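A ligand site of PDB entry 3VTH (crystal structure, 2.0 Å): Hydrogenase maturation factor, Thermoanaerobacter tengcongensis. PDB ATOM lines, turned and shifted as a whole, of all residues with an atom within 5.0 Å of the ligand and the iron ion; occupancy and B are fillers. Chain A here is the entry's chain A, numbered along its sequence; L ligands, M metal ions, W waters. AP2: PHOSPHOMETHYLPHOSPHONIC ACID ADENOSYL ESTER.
The backbone NH (N) of Gly 702 sits at hydrogen-bond distance from the backbone carbonyl oxygen (O) of Cys 732 (3.3 Å). A ring nitrogen (ND1) of His 487 lies close to the backbone carbonyl oxygen (O) of Cys 732 (3.2 Å). NH2 of Arg 599 lies within salt-bridge range of OE1 of Glu 617, at 3.3 Å. The side-chain hydroxyl (OG) of Ser 703 sits at hydrogen-bond distance from the backbone NH (N) of Asp 507, at 3.4 Å. The side-chain carboxylate of Glu 617 is in hydrogen-bond range of the side-chain hydroxyl of Tyr 409 (2.8 Å). O of Asp 507 is in hydrogen-bond range of N of Gly 598, at 2.9 Å. NE2 of Gln 705 lies close to ND2 of Asn 733 (2.9 Å). OD1 of Asn 706 lies within hydrogen-bond range of N of Leu 709 (3.0 Å).
Water W3 lies within hydrogen-bond range of a nitrogen (N3) of the ligand, the side-chain hydroxyl (OG) of Ser 703 and the backbone NH (N) of Gly 598. Water W4 bridges a nitrogen (N7) of the ligand (2.7 Å) and the side-chain sulfur of Met 622 (3.3 Å). Water W1 lies within hydrogen-bond range of an oxygen (O2') of the ligand, the backbone carbonyl oxygen (O) of Gly 598 and the guanidinium group (NH2) of Arg 599. Water W2 bridges OE2 of Glu 617 and O1B of the ligand.
The iron ion is bound by O2B of the ligand, at 2.0 Å. OD2 of Asp 507 is bound to the iron ion (2.1 Å). NE2 of His 487 is bound to the iron ion. The iron ion is bound by NE2 of His 483, at 2.2 Å. O2A of the ligand binds the iron ion (2.2 Å). The side-chain carboxylate (OD1) of Asp 734 binds the iron ion (2.2 Å). The iron ion has six donor atoms within binding distance.
Residues that only touch the ligand: Glu 617 (3.1 Å), Tyr 409 (3.1 Å), Asn 733 (3.2 Å), Gly 598 (3.3 Å), Gln 705 (3.5 Å), Ala 621 (3.5 Å), Phe 601 (3.6 Å), Arg 599 (3.7 Å) and Gly 618 (3.9 Å). The nearest printed residue that does not touch the ligand is Met 622 (4.1 Å).
O3B of the ligand is in hydrogen-bond range of OG1 of Thr 509 (3.1 Å). N of Ser 703 is in hydrogen-bond range of O4' of the ligand, 3.5 Å away. The backbone NH (N) of Asp 734 is in hydrogen-bond range of an oxygen (O1A) of the ligand (3.0 Å). O3B of the ligand sits close to O of Thr 509, 2.8 Å away. N6 of the ligand sits at hydrogen-bond distance from OE1 of Glu 625, 2.8 Å away. An oxygen (O2A) of the ligand sits close to the backbone NH (N) of Gly 702 (3.2 Å). ND2 of Asn 706 lies within hydrogen-bond range of N1 of the ligand, 2.9 Å away. N of Gly 508 is in hydrogen-bond range of O1B of the ligand (2.8 Å). The backbone NH (N) of Thr 509 sits at hydrogen-bond distance from an oxygen (O1B) of the ligand.
The nearest printed residue that does not touch the iron ion is Thr 509 (4.6 Å).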
ATOM      1  N   TYR A 409      20.234 -27.813 -23.073  1.00  0.00           N
ATOM      2  CA  TYR A 409      20.641 -29.014 -22.358  1.00  0.00           C
ATOM      3  C   TYR A 409      19.537 -29.496 -21.435  1.00  0.00           C
ATOM      4  O   TYR A 409      18.857 -28.687 -20.800  1.00  0.00           O
ATOM      5  CB  TYR A 409      21.862 -28.744 -21.479  1.00  0.00           C
ATOM      6  CG  TYR A 409      23.128 -28.441 -22.241  1.00  0.00           C
ATOM      7  CD1 TYR A 409      23.824 -29.442 -22.917  1.00  0.00           C
ATOM      8  CD2 TYR A 409      23.639 -27.135 -22.274  1.00  0.00           C
ATOM      9  CE1 TYR A 409      25.018 -29.162 -23.613  1.00  0.00           C
ATOM     10  CE2 TYR A 409      24.823 -26.845 -22.973  1.00  0.00           C
ATOM     11  CZ  TYR A 409      25.495 -27.859 -23.629  1.00  0.00           C
ATOM     12  OH  TYR A 409      26.658 -27.564 -24.312  1.00  0.00           O
ATOM     13  N   LYS A 410      19.383 -30.819 -21.354  1.00  0.00           N
ATOM     14  CA  LYS A 410      18.519 -31.419 -20.343  1.00  0.00           C
ATOM     15  C   LYS A 410      17.123 -30.787 -20.362  1.00  0.00           C
ATOM     16  O   LYS A 410      16.527 -30.491 -19.321  1.00  0.00           O
ATOM     17  CB  LYS A 410      19.149 -31.252 -18.952  1.00  0.00           C
ATOM     18  CG  LYS A 410      20.498 -31.997 -18.758  1.00  0.00           C
ATOM     19  CD  LYS A 410      21.130 -31.582 -17.415  1.00  0.00           C
ATOM     20  CE  LYS A 410      22.410 -32.366 -17.051  1.00  0.00           C
ATOM     21  NZ  LYS A 410      23.511 -32.275 -18.087  1.00  0.00           N
ATOM     22  N   TYR A 465      18.704 -21.544 -29.510  1.00  0.00           N
ATOM     23  CA  TYR A 465      18.048 -22.752 -28.960  1.00  0.00           C
ATOM     24  C   TYR A 465      16.890 -23.135 -29.865  1.00  0.00           C
ATOM     25  O   TYR A 465      16.112 -22.286 -30.287  1.00  0.00           O
ATOM     26  CB  TYR A 465      17.499 -22.493 -27.560  1.00  0.00           C
ATOM     27  CG  TYR A 465      18.518 -22.290 -26.452  1.00  0.00           C
ATOM     28  CD1 TYR A 465      19.905 -22.447 -26.680  1.00  0.00           C
ATOM     29  CD2 TYR A 465      18.094 -21.972 -25.179  1.00  0.00           C
ATOM     30  CE1 TYR A 465      20.836 -22.268 -25.610  1.00  0.00           C
ATOM     31  CE2 TYR A 465      18.989 -21.782 -24.135  1.00  0.00           C
ATOM     32  CZ  TYR A 465      20.348 -21.927 -24.368  1.00  0.00           C
ATOM     33  OH  TYR A 465      21.167 -21.721 -23.276  1.00  0.00           O
ATOM     34  N   HIS A 483      18.701 -16.402 -18.909  1.00  0.00           N
ATOM     35  CA  HIS A 483      18.954 -17.782 -18.451  1.00  0.00           C
ATOM     36  C   HIS A 483      19.204 -17.898 -16.943  1.00  0.00           C
ATOM     37  O   HIS A 483      18.636 -18.764 -16.271  1.00  0.00           O
ATOM     38  CB  HIS A 483      20.173 -18.336 -19.200  1.00  0.00           C
ATOM     39  CG  HIS A 483      20.422 -19.789 -18.976  1.00  0.00           C
ATOM     40  ND1 HIS A 483      19.796 -20.779 -19.699  1.00  0.00           N
ATOM     41  CD2 HIS A 483      21.271 -20.423 -18.118  1.00  0.00           C
ATOM     42  CE1 HIS A 483      20.230 -21.965 -19.299  1.00  0.00           C
ATOM     43  NE2 HIS A 483      21.127 -21.779 -18.347  1.00  0.00           N
ATOM     44  N   HIS A 487      17.187 -19.650 -13.710  1.00  0.00           N
ATOM     45  CA  HIS A 487      17.730 -20.593 -12.701  1.00  0.00           C
ATOM     46  C   HIS A 487      17.342 -20.128 -11.292  1.00  0.00           C
ATOM     47  O   HIS A 487      16.840 -20.930 -10.468  1.00  0.00           O
ATOM     48  CB  HIS A 487      19.274 -20.686 -12.775  1.00  0.00           C
ATOM     49  CG  HIS A 487      19.801 -21.688 -13.758  1.00  0.00           C
ATOM     50  ND1 HIS A 487      19.416 -23.016 -13.766  1.00  0.00           N
ATOM     51  CD2 HIS A 487      20.743 -21.569 -14.727  1.00  0.00           C
ATOM     52  CE1 HIS A 487      20.094 -23.663 -14.703  1.00  0.00           C
ATOM     53  NE2 HIS A 487      20.896 -22.795 -15.304  1.00  0.00           N
ATOM     54  N   ASP A 507      26.977 -21.750 -13.650  1.00  0.00           N
ATOM     55  CA  ASP A 507      26.811 -22.849 -14.614  1.00  0.00           C
ATOM     56  C   ASP A 507      27.853 -22.763 -15.738  1.00  0.00           C
ATOM     57  O   ASP A 507      28.829 -22.037 -15.593  1.00  0.00           O
ATOM     58  CB  ASP A 507      25.363 -22.973 -15.147  1.00  0.00           C
ATOM     59  CG  ASP A 507      24.903 -21.797 -16.007  1.00  0.00           C
ATOM     60  OD1 ASP A 507      25.697 -20.897 -16.391  1.00  0.00           O
ATOM     61  OD2 ASP A 507      23.682 -21.753 -16.312  1.00  0.00           O
ATOM     62  N   GLY A 508      27.646 -23.527 -16.810  1.00  0.00           N
ATOM     63  CA  GLY A 508      28.578 -23.541 -17.944  1.00  0.00           C
ATOM     64  C   GLY A 508      28.388 -22.417 -18.956  1.00  0.00           C
ATOM     65  O   GLY A 508      29.319 -21.633 -19.242  1.00  0.00           O
ATOM     66  N   THR A 509      27.192 -22.336 -19.549  1.00  0.00           N
ATOM     67  CA  THR A 509      26.941 -21.317 -20.563  1.00  0.00           C
ATOM     68  C   THR A 509      25.489 -20.920 -20.564  1.00  0.00           C
ATOM     69  O   THR A 509      24.598 -21.753 -20.672  1.00  0.00           O
ATOM     70  CB  THR A 509      27.239 -21.828 -22.017  1.00  0.00           C
ATOM     71  OG1 THR A 509      26.557 -23.067 -22.230  1.00  0.00           O
ATOM     72  CG2 THR A 509      28.712 -22.035 -22.236  1.00  0.00           C
ATOM     73  N   GLY A 510      25.250 -19.629 -20.476  1.00  0.00           N
ATOM     74  CA  GLY A 510      23.920 -19.089 -20.667  1.00  0.00           C
ATOM     75  C   GLY A 510      24.153 -17.793 -21.386  1.00  0.00           C
ATOM     76  O   GLY A 510      25.186 -17.149 -21.201  1.00  0.00           O
ATOM     77  N   GLY A 598      31.516 -23.073 -15.020  1.00  0.00           N
ATOM     78  CA  GLY A 598      31.831 -24.319 -15.748  1.00  0.00           C
ATOM     79  C   GLY A 598      33.168 -24.275 -16.481  1.00  0.00           C
ATOM     80  O   GLY A 598      33.966 -25.213 -16.399  1.00  0.00           O
ATOM     81  N   ARG A 599      33.411 -23.185 -17.209  1.00  0.00           N
ATOM     82  CA  ARG A 599      34.667 -23.028 -17.930  1.00  0.00           C
ATOM     83  C   ARG A 599      35.837 -22.842 -16.963  1.00  0.00           C
ATOM     84  O   ARG A 599      36.945 -23.306 -17.230  1.00  0.00           O
ATOM     85  CB  ARG A 599      34.623 -21.872 -18.948  1.00  0.00           C
ATOM     86  CG  ARG A 599      33.544 -21.979 -20.069  1.00  0.00           C
ATOM     87  CD  ARG A 599      33.697 -23.169 -21.050  1.00  0.00           C
ATOM     88  NE  ARG A 599      33.423 -24.447 -20.379  1.00  0.00           N
ATOM     89  CZ  ARG A 599      32.209 -24.981 -20.217  1.00  0.00           C
ATOM     90  NH1 ARG A 599      31.131 -24.380 -20.702  1.00  0.00           N
ATOM     91  NH2 ARG A 599      32.083 -26.126 -19.568  1.00  0.00           N
ATOM     92  N   PHE A 601      36.075 -24.240 -13.996  1.00  0.00           N
ATOM     93  CA  PHE A 601      36.383 -25.631 -13.641  1.00  0.00           C
ATOM     94  C   PHE A 601      37.167 -26.353 -14.736  1.00  0.00           C
ATOM     95  O   PHE A 601      38.154 -27.020 -14.437  1.00  0.00           O
ATOM     96  CB  PHE A 601      35.097 -26.425 -13.296  1.00  0.00           C
ATOM     97  CG  PHE A 601      34.768 -26.407 -11.832  1.00  0.00           C
ATOM     98  CD1 PHE A 601      34.878 -27.577 -11.078  1.00  0.00           C
ATOM     99  CD2 PHE A 601      34.339 -25.233 -11.209  1.00  0.00           C
ATOM    100  CE1 PHE A 601      34.549 -27.582  -9.701  1.00  0.00           C
ATOM    101  CE2 PHE A 601      34.012 -25.228  -9.835  1.00  0.00           C
ATOM    102  CZ  PHE A 601      34.132 -26.399  -9.079  1.00  0.00           C
ATOM    103  N   GLU A 617      29.951 -32.834 -21.851  1.00  0.00           N
ATOM    104  CA  GLU A 617      29.983 -31.544 -21.168  1.00  0.00           C
ATOM    105  C   GLU A 617      29.935 -31.765 -19.641  1.00  0.00           C
ATOM    106  O   GLU A 617      29.054 -32.454 -19.138  1.00  0.00           O
ATOM    107  CB  GLU A 617      28.786 -30.705 -21.652  1.00  0.00           C
ATOM    108  CG  GLU A 617      28.626 -29.312 -21.050  1.00  0.00           C
ATOM    109  CD  GLU A 617      29.419 -28.228 -21.788  1.00  0.00           C
ATOM    110  OE1 GLU A 617      30.671 -28.208 -21.662  1.00  0.00           O
ATOM    111  OE2 GLU A 617      28.788 -27.382 -22.467  1.00  0.00           O
ATOM    112  N   GLY A 618      30.895 -31.191 -18.923  1.00  0.00           N
ATOM    113  CA  GLY A 618      30.892 -31.286 -17.472  1.00  0.00           C
ATOM    114  C   GLY A 618      31.736 -32.419 -16.925  1.00  0.00           C
ATOM    115  O   GLY A 618      31.984 -32.486 -15.721  1.00  0.00           O
ATOM    116  N   ALA A 621      34.638 -31.313 -14.859  1.00  0.00           N
ATOM    117  CA  ALA A 621      34.253 -30.750 -13.546  1.00  0.00           C
ATOM    118  C   ALA A 621      33.877 -31.847 -12.539  1.00  0.00           C
ATOM    119  O   ALA A 621      34.215 -31.744 -11.349  1.00  0.00           O
ATOM    120  CB  ALA A 621      33.150 -29.703 -13.694  1.00  0.00           C
ATOM    121  N   MET A 622      33.220 -32.901 -13.012  1.00  0.00           N
ATOM    122  CA  MET A 622      32.886 -34.059 -12.194  1.00  0.00           C
ATOM    123  C   MET A 622      34.131 -34.790 -11.689  1.00  0.00           C
ATOM    124  O   MET A 622      34.191 -35.187 -10.539  1.00  0.00           O
ATOM    125  CB  MET A 622      31.979 -35.015 -12.979  1.00  0.00           C
ATOM    126  CG  MET A 622      30.602 -34.404 -13.288  1.00  0.00           C
ATOM    127  SD  MET A 622      29.634 -35.394 -14.453  1.00  0.00           S
ATOM    128  CE  MET A 622      29.222 -36.785 -13.395  1.00  0.00           C
ATOM    129  N   GLU A 625      35.912 -32.685  -8.960  1.00  0.00           N
ATOM    130  CA  GLU A 625      35.206 -32.840  -7.680  1.00  0.00           C
ATOM    131  C   GLU A 625      35.475 -34.196  -7.030  1.00  0.00           C
ATOM    132  O   GLU A 625      35.710 -34.270  -5.816  1.00  0.00           O
ATOM    133  CB  GLU A 625      33.688 -32.632  -7.854  1.00  0.00           C
ATOM    134  CG  GLU A 625      32.914 -32.669  -6.510  1.00  0.00           C
ATOM    135  CD  GLU A 625      31.392 -32.861  -6.644  1.00  0.00           C
ATOM    136  OE1 GLU A 625      30.885 -32.946  -7.776  1.00  0.00           O
ATOM    137  OE2 GLU A 625      30.706 -32.939  -5.597  1.00  0.00           O
ATOM    138  N   GLY A 701      21.757 -23.079 -10.940  1.00  0.00           N
ATOM    139  CA  GLY A 701      22.671 -23.252 -12.061  1.00  0.00           C
ATOM    140  C   GLY A 701      23.365 -24.581 -11.882  1.00  0.00           C
ATOM    141  O   GLY A 701      23.544 -25.047 -10.758  1.00  0.00           O
ATOM    142  N   GLY A 702      23.780 -25.170 -12.993  1.00  0.00           N
ATOM    143  CA  GLY A 702      24.329 -26.521 -13.022  1.00  0.00           C
ATOM    144  C   GLY A 702      25.625 -26.740 -12.232  1.00  0.00           C
ATOM    145  O   GLY A 702      25.905 -27.871 -11.859  1.00  0.00           O
ATOM    146  N   SER A 703      26.402 -25.687 -11.957  1.00  0.00           N
ATOM    147  CA  SER A 703      27.591 -25.874 -11.104  1.00  0.00           C
ATOM    148  C   SER A 703      27.201 -26.333  -9.687  1.00  0.00           C
ATOM    149  O   SER A 703      27.995 -26.943  -8.993  1.00  0.00           O
ATOM    150  CB  SER A 703      28.436 -24.589 -11.000  1.00  0.00           C
ATOM    151  OG  SER A 703      28.904 -24.137 -12.254  1.00  0.00           O
ATOM    152  N   GLN A 705      25.264 -28.704  -8.948  1.00  0.00           N
ATOM    153  CA  GLN A 705      25.336 -30.161  -8.910  1.00  0.00           C
ATOM    154  C   GLN A 705      26.582 -30.654  -8.165  1.00  0.00           C
ATOM    155  O   GLN A 705      26.638 -31.812  -7.736  1.00  0.00           O
ATOM    156  CB  GLN A 705      25.316 -30.738 -10.312  1.00  0.00           C
ATOM    157  CG  GLN A 705      23.980 -30.527 -11.045  1.00  0.00           C
ATOM    158  CD  GLN A 705      24.095 -30.864 -12.508  1.00  0.00           C
ATOM    159  OE1 GLN A 705      24.828 -30.192 -13.262  1.00  0.00           O
ATOM    160  NE2 GLN A 705      23.382 -31.894 -12.931  1.00  0.00           N
ATOM    161  N   ASN A 706      27.571 -29.787  -8.019  1.00  0.00           N
ATOM    162  CA  ASN A 706      28.766 -30.094  -7.218  1.00  0.00           C
ATOM    163  C   ASN A 706      28.339 -30.123  -5.739  1.00  0.00           C
ATOM    164  O   ASN A 706      27.917 -29.092  -5.186  1.00  0.00           O
ATOM    165  CB  ASN A 706      29.814 -29.003  -7.466  1.00  0.00           C
ATOM    166  CG  ASN A 706      31.143 -29.296  -6.814  1.00  0.00           C
ATOM    167  OD1 ASN A 706      31.237 -29.487  -5.610  1.00  0.00           O
ATOM    168  ND2 ASN A 706      32.198 -29.352  -7.629  1.00  0.00           N
ATOM    169  N   LEU A 709      30.540 -27.671  -3.295  1.00  0.00           N
ATOM    170  CA  LEU A 709      30.159 -26.258  -3.479  1.00  0.00           C
ATOM    171  C   LEU A 709      28.821 -25.928  -2.833  1.00  0.00           C
ATOM    172  O   LEU A 709      28.696 -24.939  -2.113  1.00  0.00           O
ATOM    173  CB  LEU A 709      30.075 -25.874  -4.966  1.00  0.00           C
ATOM    174  CG  LEU A 709      31.327 -25.746  -5.825  1.00  0.00           C
ATOM    175  CD1 LEU A 709      30.961 -25.124  -7.160  1.00  0.00           C
ATOM    176  CD2 LEU A 709      32.437 -24.930  -5.136  1.00  0.00           C
ATOM    177  N   CYS A 732      18.866 -27.930 -10.300  1.00  0.00           N
ATOM    178  CA  CYS A 732      19.567 -26.668 -10.414  1.00  0.00           C
ATOM    179  C   CYS A 732      20.219 -26.580 -11.792  1.00  0.00           C
ATOM    180  O   CYS A 732      20.631 -25.510 -12.220  1.00  0.00           O
ATOM    181  CB  CYS A 732      20.611 -26.495  -9.288  1.00  0.00           C
ATOM    182  SG  CYS A 732      21.929 -27.753  -9.305  1.00  0.00           S
ATOM    183  N   ASN A 733      20.307 -27.715 -12.495  1.00  0.00           N
ATOM    184  CA  ASN A 733      20.771 -27.709 -13.894  1.00  0.00           C
ATOM    185  C   ASN A 733      19.664 -27.240 -14.841  1.00  0.00           C
ATOM    186  O   ASN A 733      18.591 -26.865 -14.383  1.00  0.00           O
ATOM    187  CB  ASN A 733      21.365 -29.057 -14.306  1.00  0.00           C
ATOM    188  CG  ASN A 733      20.331 -30.186 -14.325  1.00  0.00           C
ATOM    189  OD1 ASN A 733      19.224 -30.047 -14.865  1.00  0.00           O
ATOM    190  ND2 ASN A 733      20.701 -31.328 -13.736  1.00  0.00           N
ATOM    191  N   ASP A 734      19.930 -27.248 -16.142  1.00  0.00           N
ATOM    192  CA  ASP A 734      18.967 -26.674 -17.097  1.00  0.00           C
ATOM    193  C   ASP A 734      17.609 -27.366 -17.174  1.00  0.00           C
ATOM    194  O   ASP A 734      16.673 -26.817 -17.765  1.00  0.00           O
ATOM    195  CB  ASP A 734      19.594 -26.556 -18.493  1.00  0.00           C
ATOM    196  CG  ASP A 734      20.532 -25.362 -18.608  1.00  0.00           C
ATOM    197  OD1 ASP A 734      20.749 -24.678 -17.584  1.00  0.00           O
ATOM    198  OD2 ASP A 734      21.051 -25.099 -19.714  1.00  0.00           O
ATOM    199  N   ILE A 737      15.114 -24.931 -15.693  1.00  0.00           N
ATOM    200  CA  ILE A 737      14.950 -23.605 -16.315  1.00  0.00           C
ATOM    201  C   ILE A 737      13.480 -23.251 -16.648  1.00  0.00           C
ATOM    202  O   ILE A 737      13.048 -22.149 -16.403  1.00  0.00           O
ATOM    203  CB  ILE A 737      15.841 -23.499 -17.574  1.00  0.00           C
ATOM    204  CG1 ILE A 737      17.328 -23.288 -17.182  1.00  0.00           C
ATOM    205  CG2 ILE A 737      15.355 -22.459 -18.560  1.00  0.00           C
ATOM    206  CD1 ILE A 737      17.673 -21.890 -16.628  1.00  0.00           C
HETATM  207  PB  AP2 L   1      24.311 -24.397 -19.161  1.00  0.00           P
HETATM  208  O1B AP2 L   1      25.736 -24.356 -18.660  1.00  0.00           O
HETATM  209  O2B AP2 L   1      23.363 -23.400 -18.578  1.00  0.00           O
HETATM  210  O3B AP2 L   1      24.250 -24.517 -20.670  1.00  0.00           O
HETATM  211  C3A AP2 L   1      23.741 -26.017 -18.578  1.00  0.00           C
HETATM  212  PA  AP2 L   1      23.580 -26.177 -16.779  1.00  0.00           P
HETATM  213  O1A AP2 L   1      22.863 -27.510 -16.677  1.00  0.00           O
HETATM  214  O2A AP2 L   1      23.028 -24.974 -16.055  1.00  0.00           O
HETATM  215  O5' AP2 L   1      25.104 -26.328 -16.256  1.00  0.00           O
HETATM  216  C5' AP2 L   1      25.801 -27.523 -16.576  1.00  0.00           C
HETATM  217  C4' AP2 L   1      27.253 -27.221 -16.294  1.00  0.00           C
HETATM  218  O4' AP2 L   1      27.481 -27.196 -14.882  1.00  0.00           O
HETATM  219  C3' AP2 L   1      28.184 -28.299 -16.816  1.00  0.00           C
HETATM  220  O3' AP2 L   1      28.400 -28.154 -18.228  1.00  0.00           O
HETATM  221  C2' AP2 L   1      29.410 -28.035 -15.976  1.00  0.00           C
HETATM  222  O2' AP2 L   1      30.115 -26.956 -16.602  1.00  0.00           O
HETATM  223  C1' AP2 L   1      28.824 -27.595 -14.619  1.00  0.00           C
HETATM  224  N9  AP2 L   1      28.921 -28.771 -13.703  1.00  0.00           N
HETATM  225  C8  AP2 L   1      28.280 -29.960 -13.817  1.00  0.00           C
HETATM  226  N7  AP2 L   1      28.643 -30.813 -12.834  1.00  0.00           N
HETATM  227  C5  AP2 L   1      29.529 -30.170 -12.045  1.00  0.00           C
HETATM  228  C6  AP2 L   1      30.307 -30.492 -10.826  1.00  0.00           C
HETATM  229  N6  AP2 L   1      30.211 -31.697 -10.215  1.00  0.00           N
HETATM  230  N1  AP2 L   1      31.137 -29.529 -10.347  1.00  0.00           N
HETATM  231  C2  AP2 L   1      31.249 -28.310 -10.918  1.00  0.00           C
HETATM  232  N3  AP2 L   1      30.571 -27.956 -12.037  1.00  0.00           N
HETATM  233  C4  AP2 L   1      29.716 -28.830 -12.634  1.00  0.00           C
HETATM  234 FE    FE M   1      22.231 -23.128 -17.000  1.00  0.00          FE
HETATM  235  O   HOH W   1      32.762 -27.746 -16.715  1.00  0.00           O
HETATM  236  O   HOH W   2      27.783 -25.927 -20.381  1.00  0.00           O
HETATM  237  O   HOH W   3      31.114 -25.544 -12.654  1.00  0.00           O
HETATM  238  O   HOH W   4      27.428 -33.172 -13.300  1.00  0.00           O
